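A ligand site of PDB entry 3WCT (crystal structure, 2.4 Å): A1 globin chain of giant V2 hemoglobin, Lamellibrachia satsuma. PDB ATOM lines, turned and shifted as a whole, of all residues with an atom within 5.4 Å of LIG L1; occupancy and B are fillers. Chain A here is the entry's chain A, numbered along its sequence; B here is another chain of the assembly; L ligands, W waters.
NE2 of His 94 of chain A binds FE1 of LIG L1 (2.1 Å). The side-chain hydroxyl (OG) of Ser 48 is in hydrogen-bond range of an oxygen (O3) of LIG L1, at 2.7 Å. An oxygen (O1) of LIG L1 sits at hydrogen-bond distance from a ring nitrogen (NE2) of His 94 of chain B, 3.3 Å away. The side-chain amide nitrogen (NE2) of Gln 98 of chain B lies within hydrogen-bond range of an oxygen (O2) of LIG L1, 3.1 Å away. O2 of LG2 L2 lies within hydrogen-bond range of NE2 of His 62 (2.9 Å). The guanidinium group (NH2) of Arg 97 is in salt-bridge range of an oxygen (O3) of LIG L1 (3.9 Å).
O1 of LG2 L2 binds FE1 of LIG L1, at 1.8 Å.
O of Leu 90 lies within hydrogen-bond range of ND1 of His 94 of chain A. The backbone carbonyl oxygen of Phe 104 lies within hydrogen-bond range of the side-chain hydroxyl of Tyr 132 (2.5 Å).
Leu 45 touches LIG L1. Phe 46 touches LIG L1. CG1 of Val 49 touches C34 of LIG L1 (3.5 Å). CE1 of His 62 touches C30 of LIG L1, at 3.6 Å. O of Arg 65 touches C9 of LIG L1, 3.5 Å away. Val 66 touches LIG L1. NE2 of Gln 93 touches C11 of LIG L1, at 3.7 Å. CD1 of Leu 99 touches C4 of LIG L1 (3.7 Å). Asn 103 touches LIG L1 (O to C24, 3.5 Å). Phe 104 touches LIG L1. Phe 107 touches LIG L1 (CE1 to C18, 3.4 Å). OH of Tyr 132 touches C19 of LIG L1, at 3.8 Å. Ile 135 touches LIG L1. Ile 139 touches LIG L1 (CD1 to C19, 3.6 Å). Within 4 Å of LIG L1: Leu 45, Phe 46, Ser 48, Val 49, His 62, Arg 65, Val 66, Gln 93, His 94 of chain A, Arg 97, Leu 99, Asn 103, Phe 104, Phe 107, Tyr 132, Ile 135, Ile 139, His 94 of chain B and Gln 98 of chain B. The nearest printed residue that does not touch LIG L1 is Leu 90 (4.01 Å).
Water W1 lies within hydrogen-bond range of a ring nitrogen (ND1) of His 62 (2.8 Å), the guanidinium group of Arg 65 (2.9 Å) and an oxygen (O4) of LIG L1 (3.3 Å).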
ATOM      1  N   TRP A  32     -15.185   3.905  -3.852  1.00  0.00           N
ATOM      2  CA  TRP A  32     -14.334   2.764  -3.580  1.00  0.00           C
ATOM      3  C   TRP A  32     -14.085   2.448  -2.115  1.00  0.00           C
ATOM      4  O   TRP A  32     -13.801   1.309  -1.766  1.00  0.00           O
ATOM      5  CB  TRP A  32     -13.019   2.907  -4.349  1.00  0.00           C
ATOM      6  CG  TRP A  32     -13.274   2.618  -5.776  1.00  0.00           C
ATOM      7  CD1 TRP A  32     -13.560   3.520  -6.758  1.00  0.00           C
ATOM      8  CD2 TRP A  32     -13.412   1.319  -6.361  1.00  0.00           C
ATOM      9  NE1 TRP A  32     -13.885   2.863  -7.916  1.00  0.00           N
ATOM     10  CE2 TRP A  32     -13.804   1.517  -7.698  1.00  0.00           C
ATOM     11  CE3 TRP A  32     -13.252   0.019  -5.880  1.00  0.00           C
ATOM     12  CZ2 TRP A  32     -14.044   0.444  -8.576  1.00  0.00           C
ATOM     13  CZ3 TRP A  32     -13.490  -1.057  -6.748  1.00  0.00           C
ATOM     14  CH2 TRP A  32     -13.882  -0.826  -8.086  1.00  0.00           C
ATOM     15  N   ALA A  42     -13.467  -8.057  -1.398  1.00  0.00           N
ATOM     16  CA  ALA A  42     -13.323  -7.587  -2.774  1.00  0.00           C
ATOM     17  C   ALA A  42     -12.031  -6.803  -2.982  1.00  0.00           C
ATOM     18  O   ALA A  42     -11.534  -6.696  -4.106  1.00  0.00           O
ATOM     19  CB  ALA A  42     -14.520  -6.728  -3.154  1.00  0.00           C
ATOM     20  N   LEU A  45      -9.152  -8.312  -4.872  1.00  0.00           N
ATOM     21  CA  LEU A  45      -9.364  -8.473  -6.312  1.00  0.00           C
ATOM     22  C   LEU A  45      -8.660  -7.402  -7.155  1.00  0.00           C
ATOM     23  O   LEU A  45      -8.609  -7.522  -8.379  1.00  0.00           O
ATOM     24  CB  LEU A  45     -10.866  -8.448  -6.628  1.00  0.00           C
ATOM     25  CG  LEU A  45     -11.741  -9.386  -5.797  1.00  0.00           C
ATOM     26  CD1 LEU A  45     -13.213  -9.097  -6.050  1.00  0.00           C
ATOM     27  CD2 LEU A  45     -11.411 -10.838  -6.149  1.00  0.00           C
ATOM     28  N   PHE A  46      -8.112  -6.375  -6.499  1.00  0.00           N
ATOM     29  CA  PHE A  46      -7.467  -5.280  -7.223  1.00  0.00           C
ATOM     30  C   PHE A  46      -5.995  -5.073  -6.945  1.00  0.00           C
ATOM     31  O   PHE A  46      -5.500  -3.947  -6.998  1.00  0.00           O
ATOM     32  CB  PHE A  46      -8.220  -3.981  -6.953  1.00  0.00           C
ATOM     33  CG  PHE A  46      -9.670  -4.048  -7.311  1.00  0.00           C
ATOM     34  CD1 PHE A  46     -10.119  -3.557  -8.543  1.00  0.00           C
ATOM     35  CD2 PHE A  46     -10.596  -4.616  -6.438  1.00  0.00           C
ATOM     36  CE1 PHE A  46     -11.463  -3.651  -8.893  1.00  0.00           C
ATOM     37  CE2 PHE A  46     -11.949  -4.706  -6.785  1.00  0.00           C
ATOM     38  CZ  PHE A  46     -12.378  -4.225  -8.014  1.00  0.00           C
ATOM     39  N   SER A  48      -3.761  -5.807  -8.788  1.00  0.00           N
ATOM     40  CA  SER A  48      -3.170  -5.390 -10.055  1.00  0.00           C
ATOM     41  C   SER A  48      -3.127  -3.868 -10.205  1.00  0.00           C
ATOM     42  O   SER A  48      -2.337  -3.344 -11.004  1.00  0.00           O
ATOM     43  CB  SER A  48      -3.939  -6.014 -11.231  1.00  0.00           C
ATOM     44  OG  SER A  48      -5.342  -5.815 -11.141  1.00  0.00           O
ATOM     45  N   VAL A  49      -3.961  -3.155  -9.440  1.00  0.00           N
ATOM     46  CA  VAL A  49      -3.966  -1.683  -9.454  1.00  0.00           C
ATOM     47  C   VAL A  49      -3.589  -1.111  -8.099  1.00  0.00           C
ATOM     48  O   VAL A  49      -3.974   0.010  -7.751  1.00  0.00           O
ATOM     49  CB  VAL A  49      -5.330  -1.086  -9.875  1.00  0.00           C
ATOM     50  CG1 VAL A  49      -5.496  -1.210 -11.379  1.00  0.00           C
ATOM     51  CG2 VAL A  49      -6.466  -1.758  -9.133  1.00  0.00           C
ATOM     52  N   HIS A  62      -7.098   3.836 -11.527  1.00  0.00           N
ATOM     53  CA  HIS A  62      -8.162   2.854 -11.665  1.00  0.00           C
ATOM     54  C   HIS A  62      -9.514   3.492 -11.322  1.00  0.00           C
ATOM     55  O   HIS A  62     -10.505   3.270 -12.026  1.00  0.00           O
ATOM     56  CB  HIS A  62      -7.932   1.666 -10.735  1.00  0.00           C
ATOM     57  CG  HIS A  62      -9.079   0.707 -10.694  1.00  0.00           C
ATOM     58  ND1 HIS A  62      -9.397  -0.117 -11.754  1.00  0.00           N
ATOM     59  CD2 HIS A  62     -10.014   0.472  -9.747  1.00  0.00           C
ATOM     60  CE1 HIS A  62     -10.468  -0.816 -11.457  1.00  0.00           C
ATOM     61  NE2 HIS A  62     -10.873  -0.481 -10.249  1.00  0.00           N
ATOM     62  N   ARG A  65     -10.563   5.677 -14.083  1.00  0.00           N
ATOM     63  CA  ARG A  65     -11.070   4.895 -15.212  1.00  0.00           C
ATOM     64  C   ARG A  65     -12.490   4.370 -14.967  1.00  0.00           C
ATOM     65  O   ARG A  65     -13.333   4.399 -15.856  1.00  0.00           O
ATOM     66  CB  ARG A  65     -10.120   3.747 -15.560  1.00  0.00           C
ATOM     67  CG  ARG A  65      -8.829   4.172 -16.245  1.00  0.00           C
ATOM     68  CD  ARG A  65      -8.055   2.987 -16.851  1.00  0.00           C
ATOM     69  NE  ARG A  65      -7.396   2.141 -15.858  1.00  0.00           N
ATOM     70  CZ  ARG A  65      -6.258   2.448 -15.239  1.00  0.00           C
ATOM     71  NH1 ARG A  65      -5.631   3.592 -15.503  1.00  0.00           N
ATOM     72  NH2 ARG A  65      -5.752   1.610 -14.335  1.00  0.00           N
ATOM     73  N   VAL A  66     -12.763   3.903 -13.762  1.00  0.00           N
ATOM     74  CA  VAL A  66     -14.089   3.378 -13.444  1.00  0.00           C
ATOM     75  C   VAL A  66     -15.218   4.428 -13.427  1.00  0.00           C
ATOM     76  O   VAL A  66     -16.283   4.213 -14.003  1.00  0.00           O
ATOM     77  CB  VAL A  66     -14.076   2.643 -12.082  1.00  0.00           C
ATOM     78  CG1 VAL A  66     -15.502   2.236 -11.691  1.00  0.00           C
ATOM     79  CG2 VAL A  66     -13.154   1.425 -12.186  1.00  0.00           C
ATOM     80  N   GLY A  69     -15.875   5.399 -16.643  1.00  0.00           N
ATOM     81  CA  GLY A  69     -16.707   4.411 -17.313  1.00  0.00           C
ATOM     82  C   GLY A  69     -18.170   4.646 -16.992  1.00  0.00           C
ATOM     83  O   GLY A  69     -19.004   4.671 -17.885  1.00  0.00           O
ATOM     84  N   LEU A  70     -18.468   4.830 -15.709  1.00  0.00           N
ATOM     85  CA  LEU A  70     -19.830   5.095 -15.264  1.00  0.00           C
ATOM     86  C   LEU A  70     -20.395   6.322 -15.979  1.00  0.00           C
ATOM     87  O   LEU A  70     -21.538   6.328 -16.434  1.00  0.00           O
ATOM     88  CB  LEU A  70     -19.846   5.331 -13.754  1.00  0.00           C
ATOM     89  CG  LEU A  70     -19.995   4.093 -12.854  1.00  0.00           C
ATOM     90  CD1 LEU A  70     -19.758   4.483 -11.391  1.00  0.00           C
ATOM     91  CD2 LEU A  70     -21.384   3.512 -13.054  1.00  0.00           C
ATOM     92  N   ARG A  72     -19.457   7.768 -18.971  1.00  0.00           N
ATOM     93  CA  ARG A  72     -19.724   7.608 -20.408  1.00  0.00           C
ATOM     94  C   ARG A  72     -20.930   6.697 -20.638  1.00  0.00           C
ATOM     95  O   ARG A  72     -21.732   6.923 -21.552  1.00  0.00           O
ATOM     96  CB  ARG A  72     -18.488   7.066 -21.134  1.00  0.00           C
ATOM     97  CG  ARG A  72     -18.199   5.617 -20.861  1.00  0.00           C
ATOM     98  CD  ARG A  72     -16.823   5.214 -21.374  1.00  0.00           C
ATOM     99  NE  ARG A  72     -16.797   3.774 -21.614  1.00  0.00           N
ATOM    100  CZ  ARG A  72     -15.760   2.978 -21.367  1.00  0.00           C
ATOM    101  NH1 ARG A  72     -14.646   3.472 -20.846  1.00  0.00           N
ATOM    102  NH2 ARG A  72     -15.866   1.688 -21.624  1.00  0.00           N
ATOM    103  N   LEU A  90     -17.167  -3.218 -22.171  1.00  0.00           N
ATOM    104  CA  LEU A  90     -16.837  -3.347 -20.765  1.00  0.00           C
ATOM    105  C   LEU A  90     -16.965  -4.799 -20.335  1.00  0.00           C
ATOM    106  O   LEU A  90     -16.294  -5.236 -19.411  1.00  0.00           O
ATOM    107  CB  LEU A  90     -17.750  -2.464 -19.895  1.00  0.00           C
ATOM    108  CG  LEU A  90     -17.600  -0.941 -20.061  1.00  0.00           C
ATOM    109  CD1 LEU A  90     -18.632  -0.250 -19.200  1.00  0.00           C
ATOM    110  CD2 LEU A  90     -16.185  -0.496 -19.684  1.00  0.00           C
ATOM    111  N   GLN A  93     -13.902  -6.902 -21.056  1.00  0.00           N
ATOM    112  CA  GLN A  93     -12.772  -6.551 -20.195  1.00  0.00           C
ATOM    113  C   GLN A  93     -12.867  -7.199 -18.812  1.00  0.00           C
ATOM    114  O   GLN A  93     -11.851  -7.432 -18.169  1.00  0.00           O
ATOM    115  CB  GLN A  93     -12.651  -5.024 -20.040  1.00  0.00           C
ATOM    116  CG  GLN A  93     -12.302  -4.277 -21.316  1.00  0.00           C
ATOM    117  CD  GLN A  93     -12.527  -2.768 -21.199  1.00  0.00           C
ATOM    118  OE1 GLN A  93     -13.602  -2.319 -20.801  1.00  0.00           O
ATOM    119  NE2 GLN A  93     -11.508  -1.981 -21.542  1.00  0.00           N
ATOM    120  N   HIS A  94     -14.095  -7.473 -18.354  1.00  0.00           N
ATOM    121  CA  HIS A  94     -14.271  -8.094 -17.039  1.00  0.00           C
ATOM    122  C   HIS A  94     -14.409  -9.624 -17.083  1.00  0.00           C
ATOM    123  O   HIS A  94     -14.027 -10.296 -16.128  1.00  0.00           O
ATOM    124  CB  HIS A  94     -15.496  -7.477 -16.325  1.00  0.00           C
ATOM    125  CG  HIS A  94     -15.288  -6.070 -15.873  1.00  0.00           C
ATOM    126  ND1 HIS A  94     -15.256  -4.998 -16.743  1.00  0.00           N
ATOM    127  CD2 HIS A  94     -15.106  -5.545 -14.635  1.00  0.00           C
ATOM    128  CE1 HIS A  94     -15.073  -3.882 -16.064  1.00  0.00           C
ATOM    129  NE2 HIS A  94     -14.973  -4.186 -14.773  1.00  0.00           N
ATOM    130  N   ARG A  97     -11.705 -12.206 -16.022  1.00  0.00           N
ATOM    131  CA  ARG A  97     -11.211 -12.053 -14.665  1.00  0.00           C
ATOM    132  C   ARG A  97     -11.960 -12.915 -13.659  1.00  0.00           C
ATOM    133  O   ARG A  97     -11.684 -12.868 -12.454  1.00  0.00           O
ATOM    134  CB  ARG A  97     -11.262 -10.596 -14.231  1.00  0.00           C
ATOM    135  CG  ARG A  97     -10.679  -9.625 -15.248  1.00  0.00           C
ATOM    136  CD  ARG A  97     -10.332  -8.309 -14.601  1.00  0.00           C
ATOM    137  NE  ARG A  97      -8.943  -8.257 -14.146  1.00  0.00           N
ATOM    138  CZ  ARG A  97      -7.923  -7.833 -14.894  1.00  0.00           C
ATOM    139  NH1 ARG A  97      -8.145  -7.417 -16.141  1.00  0.00           N
ATOM    140  NH2 ARG A  97      -6.692  -7.798 -14.394  1.00  0.00           N
ATOM    141  N   LEU A  99     -14.832 -12.751 -12.222  1.00  0.00           N
ATOM    142  CA  LEU A  99     -15.354 -11.969 -11.105  1.00  0.00           C
ATOM    143  C   LEU A  99     -16.720 -12.485 -10.688  1.00  0.00           C
ATOM    144  O   LEU A  99     -17.564 -12.776 -11.536  1.00  0.00           O
ATOM    145  CB  LEU A  99     -15.508 -10.501 -11.492  1.00  0.00           C
ATOM    146  CG  LEU A  99     -14.309  -9.829 -12.153  1.00  0.00           C
ATOM    147  CD1 LEU A  99     -14.706  -8.416 -12.561  1.00  0.00           C
ATOM    148  CD2 LEU A  99     -13.123  -9.824 -11.188  1.00  0.00           C
ATOM    149  N   ASN A 103     -20.546  -9.156  -6.497  1.00  0.00           N
ATOM    150  CA  ASN A 103     -19.770  -7.960  -6.189  1.00  0.00           C
ATOM    151  C   ASN A 103     -20.263  -6.740  -6.977  1.00  0.00           C
ATOM    152  O   ASN A 103     -19.896  -5.620  -6.666  1.00  0.00           O
ATOM    153  CB  ASN A 103     -18.290  -8.189  -6.468  1.00  0.00           C
ATOM    154  CG  ASN A 103     -17.595  -8.903  -5.325  1.00  0.00           C
ATOM    155  OD1 ASN A 103     -16.428  -9.294  -5.437  1.00  0.00           O
ATOM    156  ND2 ASN A 103     -18.296  -9.076  -4.202  1.00  0.00           N
ATOM    157  N   PHE A 104     -21.078  -6.977  -7.989  1.00  0.00           N
ATOM    158  CA  PHE A 104     -21.631  -5.879  -8.757  1.00  0.00           C
ATOM    159  C   PHE A 104     -22.852  -5.340  -8.047  1.00  0.00           C
ATOM    160  O   PHE A 104     -23.287  -4.219  -8.300  1.00  0.00           O
ATOM    161  CB  PHE A 104     -21.975  -6.317 -10.186  1.00  0.00           C
ATOM    162  CG  PHE A 104     -20.798  -6.373 -11.101  1.00  0.00           C
ATOM    163  CD1 PHE A 104     -20.506  -5.299 -11.938  1.00  0.00           C
ATOM    164  CD2 PHE A 104     -19.931  -7.470 -11.078  1.00  0.00           C
ATOM    165  CE1 PHE A 104     -19.357  -5.320 -12.749  1.00  0.00           C
ATOM    166  CE2 PHE A 104     -18.792  -7.499 -11.878  1.00  0.00           C
ATOM    167  CZ  PHE A 104     -18.503  -6.423 -12.724  1.00  0.00           C
ATOM    168  N   PHE A 107     -21.225  -3.117  -5.543  1.00  0.00           N
ATOM    169  CA  PHE A 107     -20.795  -1.920  -6.246  1.00  0.00           C
ATOM    170  C   PHE A 107     -21.960  -0.941  -6.350  1.00  0.00           C
ATOM    171  O   PHE A 107     -21.827   0.241  -6.004  1.00  0.00           O
ATOM    172  CB  PHE A 107     -20.268  -2.294  -7.636  1.00  0.00           C
ATOM    173  CG  PHE A 107     -19.700  -1.143  -8.410  1.00  0.00           C
ATOM    174  CD1 PHE A 107     -20.522  -0.165  -8.934  1.00  0.00           C
ATOM    175  CD2 PHE A 107     -18.326  -1.049  -8.628  1.00  0.00           C
ATOM    176  CE1 PHE A 107     -19.992   0.906  -9.669  1.00  0.00           C
ATOM    177  CE2 PHE A 107     -17.785   0.015  -9.357  1.00  0.00           C
ATOM    178  CZ  PHE A 107     -18.611   0.985  -9.882  1.00  0.00           C
ATOM    179  N   TYR A 132     -29.227   0.974 -12.713  1.00  0.00           N
ATOM    180  CA  TYR A 132     -27.907   0.439 -12.445  1.00  0.00           C
ATOM    181  C   TYR A 132     -27.921  -0.988 -12.994  1.00  0.00           C
ATOM    182  O   TYR A 132     -26.992  -1.406 -13.669  1.00  0.00           O
ATOM    183  CB  TYR A 132     -27.594   0.409 -10.939  1.00  0.00           C
ATOM    184  CG  TYR A 132     -26.313  -0.333 -10.661  1.00  0.00           C
ATOM    185  CD1 TYR A 132     -26.330  -1.585 -10.035  1.00  0.00           C
ATOM    186  CD2 TYR A 132     -25.086   0.158 -11.095  1.00  0.00           C
ATOM    187  CE1 TYR A 132     -25.183  -2.315  -9.860  1.00  0.00           C
ATOM    188  CE2 TYR A 132     -23.917  -0.568 -10.924  1.00  0.00           C
ATOM    189  CZ  TYR A 132     -23.966  -1.805 -10.307  1.00  0.00           C
ATOM    190  OH  TYR A 132     -22.814  -2.546 -10.137  1.00  0.00           O
ATOM    191  N   ILE A 135     -26.858  -1.548 -16.342  1.00  0.00           N
ATOM    192  CA  ILE A 135     -25.405  -1.432 -16.454  1.00  0.00           C
ATOM    193  C   ILE A 135     -24.669  -2.709 -16.023  1.00  0.00           C
ATOM    194  O   ILE A 135     -23.780  -3.202 -16.733  1.00  0.00           O
ATOM    195  CB  ILE A 135     -24.884  -0.230 -15.617  1.00  0.00           C
ATOM    196  CG1 ILE A 135     -25.433   1.083 -16.190  1.00  0.00           C
ATOM    197  CG2 ILE A 135     -23.359  -0.225 -15.609  1.00  0.00           C
ATOM    198  CD1 ILE A 135     -24.990   2.348 -15.444  1.00  0.00           C
ATOM    199  N   ALA A 136     -25.032  -3.229 -14.857  1.00  0.00           N
ATOM    200  CA  ALA A 136     -24.409  -4.436 -14.311  1.00  0.00           C
ATOM    201  C   ALA A 136     -24.690  -5.658 -15.182  1.00  0.00           C
ATOM    202  O   ALA A 136     -23.859  -6.556 -15.303  1.00  0.00           O
ATOM    203  CB  ALA A 136     -24.893  -4.674 -12.897  1.00  0.00           C
ATOM    204  N   ILE A 139     -22.587  -5.649 -18.225  1.00  0.00           N
ATOM    205  CA  ILE A 139     -21.207  -5.983 -17.931  1.00  0.00           C
ATOM    206  C   ILE A 139     -21.056  -7.428 -17.482  1.00  0.00           C
ATOM    207  O   ILE A 139     -20.055  -8.067 -17.770  1.00  0.00           O
ATOM    208  CB  ILE A 139     -20.602  -5.031 -16.859  1.00  0.00           C
ATOM    209  CG1 ILE A 139     -20.526  -3.598 -17.412  1.00  0.00           C
ATOM    210  CG2 ILE A 139     -19.199  -5.482 -16.478  1.00  0.00           C
ATOM    211  CD1 ILE A 139     -19.966  -2.581 -16.406  1.00  0.00           C
ATOM    212  N   HIS B  94      -1.151   3.788 -18.823  1.00  0.00           N
ATOM    213  CA  HIS B  94      -2.172   2.790 -19.137  1.00  0.00           C
ATOM    214  C   HIS B  94      -2.669   3.028 -20.554  1.00  0.00           C
ATOM    215  O   HIS B  94      -2.628   2.122 -21.385  1.00  0.00           O
ATOM    216  CB  HIS B  94      -3.327   2.887 -18.140  1.00  0.00           C
ATOM    217  CG  HIS B  94      -4.391   1.840 -18.340  1.00  0.00           C
ATOM    218  ND1 HIS B  94      -5.458   2.027 -19.200  1.00  0.00           N
ATOM    219  CD2 HIS B  94      -4.554   0.614 -17.798  1.00  0.00           C
ATOM    220  CE1 HIS B  94      -6.235   0.952 -19.168  1.00  0.00           C
ATOM    221  NE2 HIS B  94      -5.705   0.082 -18.322  1.00  0.00           N
ATOM    222  N   GLN B  98      -2.620   0.754 -24.096  1.00  0.00           N
ATOM    223  CA  GLN B  98      -3.773   0.395 -24.921  1.00  0.00           C
ATOM    224  C   GLN B  98      -3.581   0.744 -26.412  1.00  0.00           C
ATOM    225  O   GLN B  98      -4.380   0.335 -27.266  1.00  0.00           O
ATOM    226  CB  GLN B  98      -5.047   1.073 -24.403  1.00  0.00           C
ATOM    227  CG  GLN B  98      -5.537   0.593 -23.041  1.00  0.00           C
ATOM    228  CD  GLN B  98      -6.765   1.369 -22.556  1.00  0.00           C
ATOM    229  OE1 GLN B  98      -6.762   2.606 -22.527  1.00  0.00           O
ATOM    230  NE2 GLN B  98      -7.822   0.644 -22.163  1.00  0.00           N
HETATM  231  C1  LIG L   1     -11.262  -2.443 -14.716  1.00  0.00           C
HETATM  232  C2  LIG L   1     -15.439  -0.225 -15.220  1.00  0.00           C
HETATM  233  C3  LIG L   1     -17.348  -2.877 -11.671  1.00  0.00           C
HETATM  234  C4  LIG L   1     -13.185  -5.271 -11.369  1.00  0.00           C
HETATM  235  C5  LIG L   1     -12.234  -1.581 -15.162  1.00  0.00           C
HETATM  236  C6  LIG L   1     -11.993  -0.602 -16.135  1.00  0.00           C
HETATM  237  C7  LIG L   1     -13.174   0.017 -16.292  1.00  0.00           C
HETATM  238  C8  LIG L   1     -14.158  -0.574 -15.401  1.00  0.00           C
HETATM  239  C9  LIG L   1     -13.472   1.176 -17.257  1.00  0.00           C
HETATM  240  C10 LIG L   1     -10.687  -0.301 -16.841  1.00  0.00           C
HETATM  241  C11 LIG L   1     -10.544  -1.082 -18.132  1.00  0.00           C
HETATM  242  C12 LIG L   1      -9.227  -0.833 -18.879  1.00  0.00           C
HETATM  243  O1  LIG L   1      -8.373  -1.757 -18.972  1.00  0.00           O
HETATM  244  O2  LIG L   1      -9.038   0.246 -19.355  1.00  0.00           O
HETATM  245  C13 LIG L   1     -16.373  -0.743 -14.297  1.00  0.00           C
HETATM  246  C14 LIG L   1     -17.726  -0.257 -14.141  1.00  0.00           C
HETATM  247  C15 LIG L   1     -18.274  -1.065 -13.072  1.00  0.00           C
HETATM  248  C16 LIG L   1     -17.242  -1.939 -12.697  1.00  0.00           C
HETATM  249  C17 LIG L   1     -18.375   0.849 -14.905  1.00  0.00           C
HETATM  250  C18 LIG L   1     -19.626  -0.900 -12.531  1.00  0.00           C
HETATM  251  C19 LIG L   1     -20.725  -1.349 -13.086  1.00  0.00           C
HETATM  252  C20 LIG L   1     -16.357  -3.759 -11.278  1.00  0.00           C
HETATM  253  C21 LIG L   1     -16.548  -4.730 -10.176  1.00  0.00           C
HETATM  254  C22 LIG L   1     -15.342  -5.471 -10.074  1.00  0.00           C
HETATM  255  C23 LIG L   1     -14.460  -4.855 -11.147  1.00  0.00           C
HETATM  256  C24 LIG L   1     -17.815  -4.876  -9.334  1.00  0.00           C
HETATM  257  C25 LIG L   1     -15.046  -6.482  -9.235  1.00  0.00           C
HETATM  258  C26 LIG L   1     -14.960  -6.729  -7.977  1.00  0.00           C
HETATM  259  C27 LIG L   1     -12.297  -4.727 -12.261  1.00  0.00           C
HETATM  260  C28 LIG L   1     -10.863  -5.184 -12.407  1.00  0.00           C
HETATM  261  C29 LIG L   1     -10.327  -4.359 -13.372  1.00  0.00           C
HETATM  262  C30 LIG L   1     -11.408  -3.433 -13.782  1.00  0.00           C
HETATM  263  C31 LIG L   1     -10.221  -6.317 -11.607  1.00  0.00           C
HETATM  264  C32 LIG L   1      -8.904  -4.386 -13.919  1.00  0.00           C
HETATM  265  C33 LIG L   1      -7.971  -3.446 -13.234  1.00  0.00           C
HETATM  266  C34 LIG L   1      -6.617  -3.463 -13.794  1.00  0.00           C
HETATM  267  O3  LIG L   1      -5.736  -4.229 -13.294  1.00  0.00           O
HETATM  268  O4  LIG L   1      -6.338  -2.723 -14.763  1.00  0.00           O
HETATM  269  N1  LIG L   1     -13.564  -1.575 -14.710  1.00  0.00           N
HETATM  270  N2  LIG L   1     -16.059  -1.748 -13.472  1.00  0.00           N
HETATM  271  N3  LIG L   1     -15.081  -3.877 -11.828  1.00  0.00           N
HETATM  272  N4  LIG L   1     -12.571  -3.714 -13.105  1.00  0.00           N
HETATM  273 FE1  LIG L   1     -14.335  -2.761 -13.314  1.00  0.00          FE
HETATM  274  O1  LG2 L   2     -13.783  -1.613 -12.060  1.00  0.00           O
HETATM  275  O2  LG2 L   2     -13.327  -1.776 -10.922  1.00  0.00           O
HETATM  276  C1  LG3 L   3      -8.589   2.972 -28.622  1.00  0.00           C
HETATM  277  C2  LG3 L   3      -8.091   7.164 -26.470  1.00  0.00           C
HETATM  278  C3  LG3 L   3      -5.622   8.878 -30.226  1.00  0.00           C
HETATM  279  C4  LG3 L   3      -5.946   4.567 -32.274  1.00  0.00           C
HETATM  280  C5  LG3 L   3      -8.686   3.960 -27.687  1.00  0.00           C
HETATM  281  C6  LG3 L   3      -9.396   3.842 -26.490  1.00  0.00           C
HETATM  282  C7  LG3 L   3      -9.239   5.024 -25.860  1.00  0.00           C
HETATM  283  C8  LG3 L   3      -8.445   5.897 -26.691  1.00  0.00           C
HETATM  284  C9  LG3 L   3      -9.803   5.441 -24.490  1.00  0.00           C
HETATM  285  C10 LG3 L   3     -10.187   2.655 -25.984  1.00  0.00           C
HETATM  286  C11 LG3 L   3      -9.331   1.745 -25.157  1.00  0.00           C
HETATM  287  C12 LG3 L   3     -10.016   0.484 -24.625  1.00  0.00           C
HETATM  288  O1  LG3 L   3      -9.572  -0.644 -24.959  1.00  0.00           O
HETATM  289  O2  LG3 L   3     -10.961   0.613 -23.918  1.00  0.00           O
HETATM  290  C13 LG3 L   3      -7.383   8.054 -27.307  1.00  0.00           C
HETATM  291  C14 LG3 L   3      -7.129   9.445 -26.991  1.00  0.00           C
HETATM  292  C15 LG3 L   3      -6.421   9.943 -28.143  1.00  0.00           C
HETATM  293  C16 LG3 L   3      -6.277   8.833 -29.010  1.00  0.00           C
HETATM  294  C17 LG3 L   3      -7.530  10.175 -25.769  1.00  0.00           C
HETATM  295  C18 LG3 L   3      -5.994  11.319 -28.295  1.00  0.00           C
HETATM  296  C19 LG3 L   3      -4.875  11.800 -27.779  1.00  0.00           C
HETATM  297  C20 LG3 L   3      -5.484   7.828 -31.105  1.00  0.00           C
HETATM  298  C21 LG3 L   3      -4.769   7.949 -32.387  1.00  0.00           C
HETATM  299  C22 LG3 L   3      -4.837   6.694 -33.009  1.00  0.00           C
HETATM  300  C23 LG3 L   3      -5.637   5.850 -32.038  1.00  0.00           C
HETATM  301  C24 LG3 L   3      -4.084   9.211 -32.919  1.00  0.00           C
HETATM  302  C25 LG3 L   3      -4.319   6.332 -34.220  1.00  0.00           C
HETATM  303  C26 LG3 L   3      -4.697   6.212 -35.445  1.00  0.00           C
HETATM  304  C27 LG3 L   3      -6.704   3.747 -31.457  1.00  0.00           C
HETATM  305  C28 LG3 L   3      -7.075   2.343 -31.835  1.00  0.00           C
HETATM  306  C29 LG3 L   3      -7.843   1.901 -30.779  1.00  0.00           C
HETATM  307  C30 LG3 L   3      -7.912   3.012 -29.801  1.00  0.00           C
HETATM  308  C31 LG3 L   3      -6.667   1.647 -33.134  1.00  0.00           C
HETATM  309  C32 LG3 L   3      -8.512   0.557 -30.643  1.00  0.00           C
HETATM  310  C33 LG3 L   3      -9.875   0.562 -31.270  1.00  0.00           C
HETATM  311  C34 LG3 L   3     -10.546  -0.732 -31.160  1.00  0.00           C
HETATM  312  O3  LG3 L   3     -11.068  -1.069 -30.058  1.00  0.00           O
HETATM  313  O4  LG3 L   3     -10.596  -1.476 -32.155  1.00  0.00           O
HETATM  314  N1  LG3 L   3      -8.081   5.221 -27.822  1.00  0.00           N
HETATM  315  N2  LG3 L   3      -6.897   7.667 -28.486  1.00  0.00           N
HETATM  316  N3  LG3 L   3      -5.978   6.535 -30.942  1.00  0.00           N
HETATM  317  N4  LG3 L   3      -7.223   4.091 -30.262  1.00  0.00           N
HETATM  318 FE1  LG3 L   3      -7.010   5.858 -29.355  1.00  0.00          FE
HETATM  319  O   HOH W   1      -8.411  -0.127 -14.352  1.00  0.00           O
HETATM  320  O   HOH W   2      -3.305  -4.308 -14.853  1.00  0.00           O
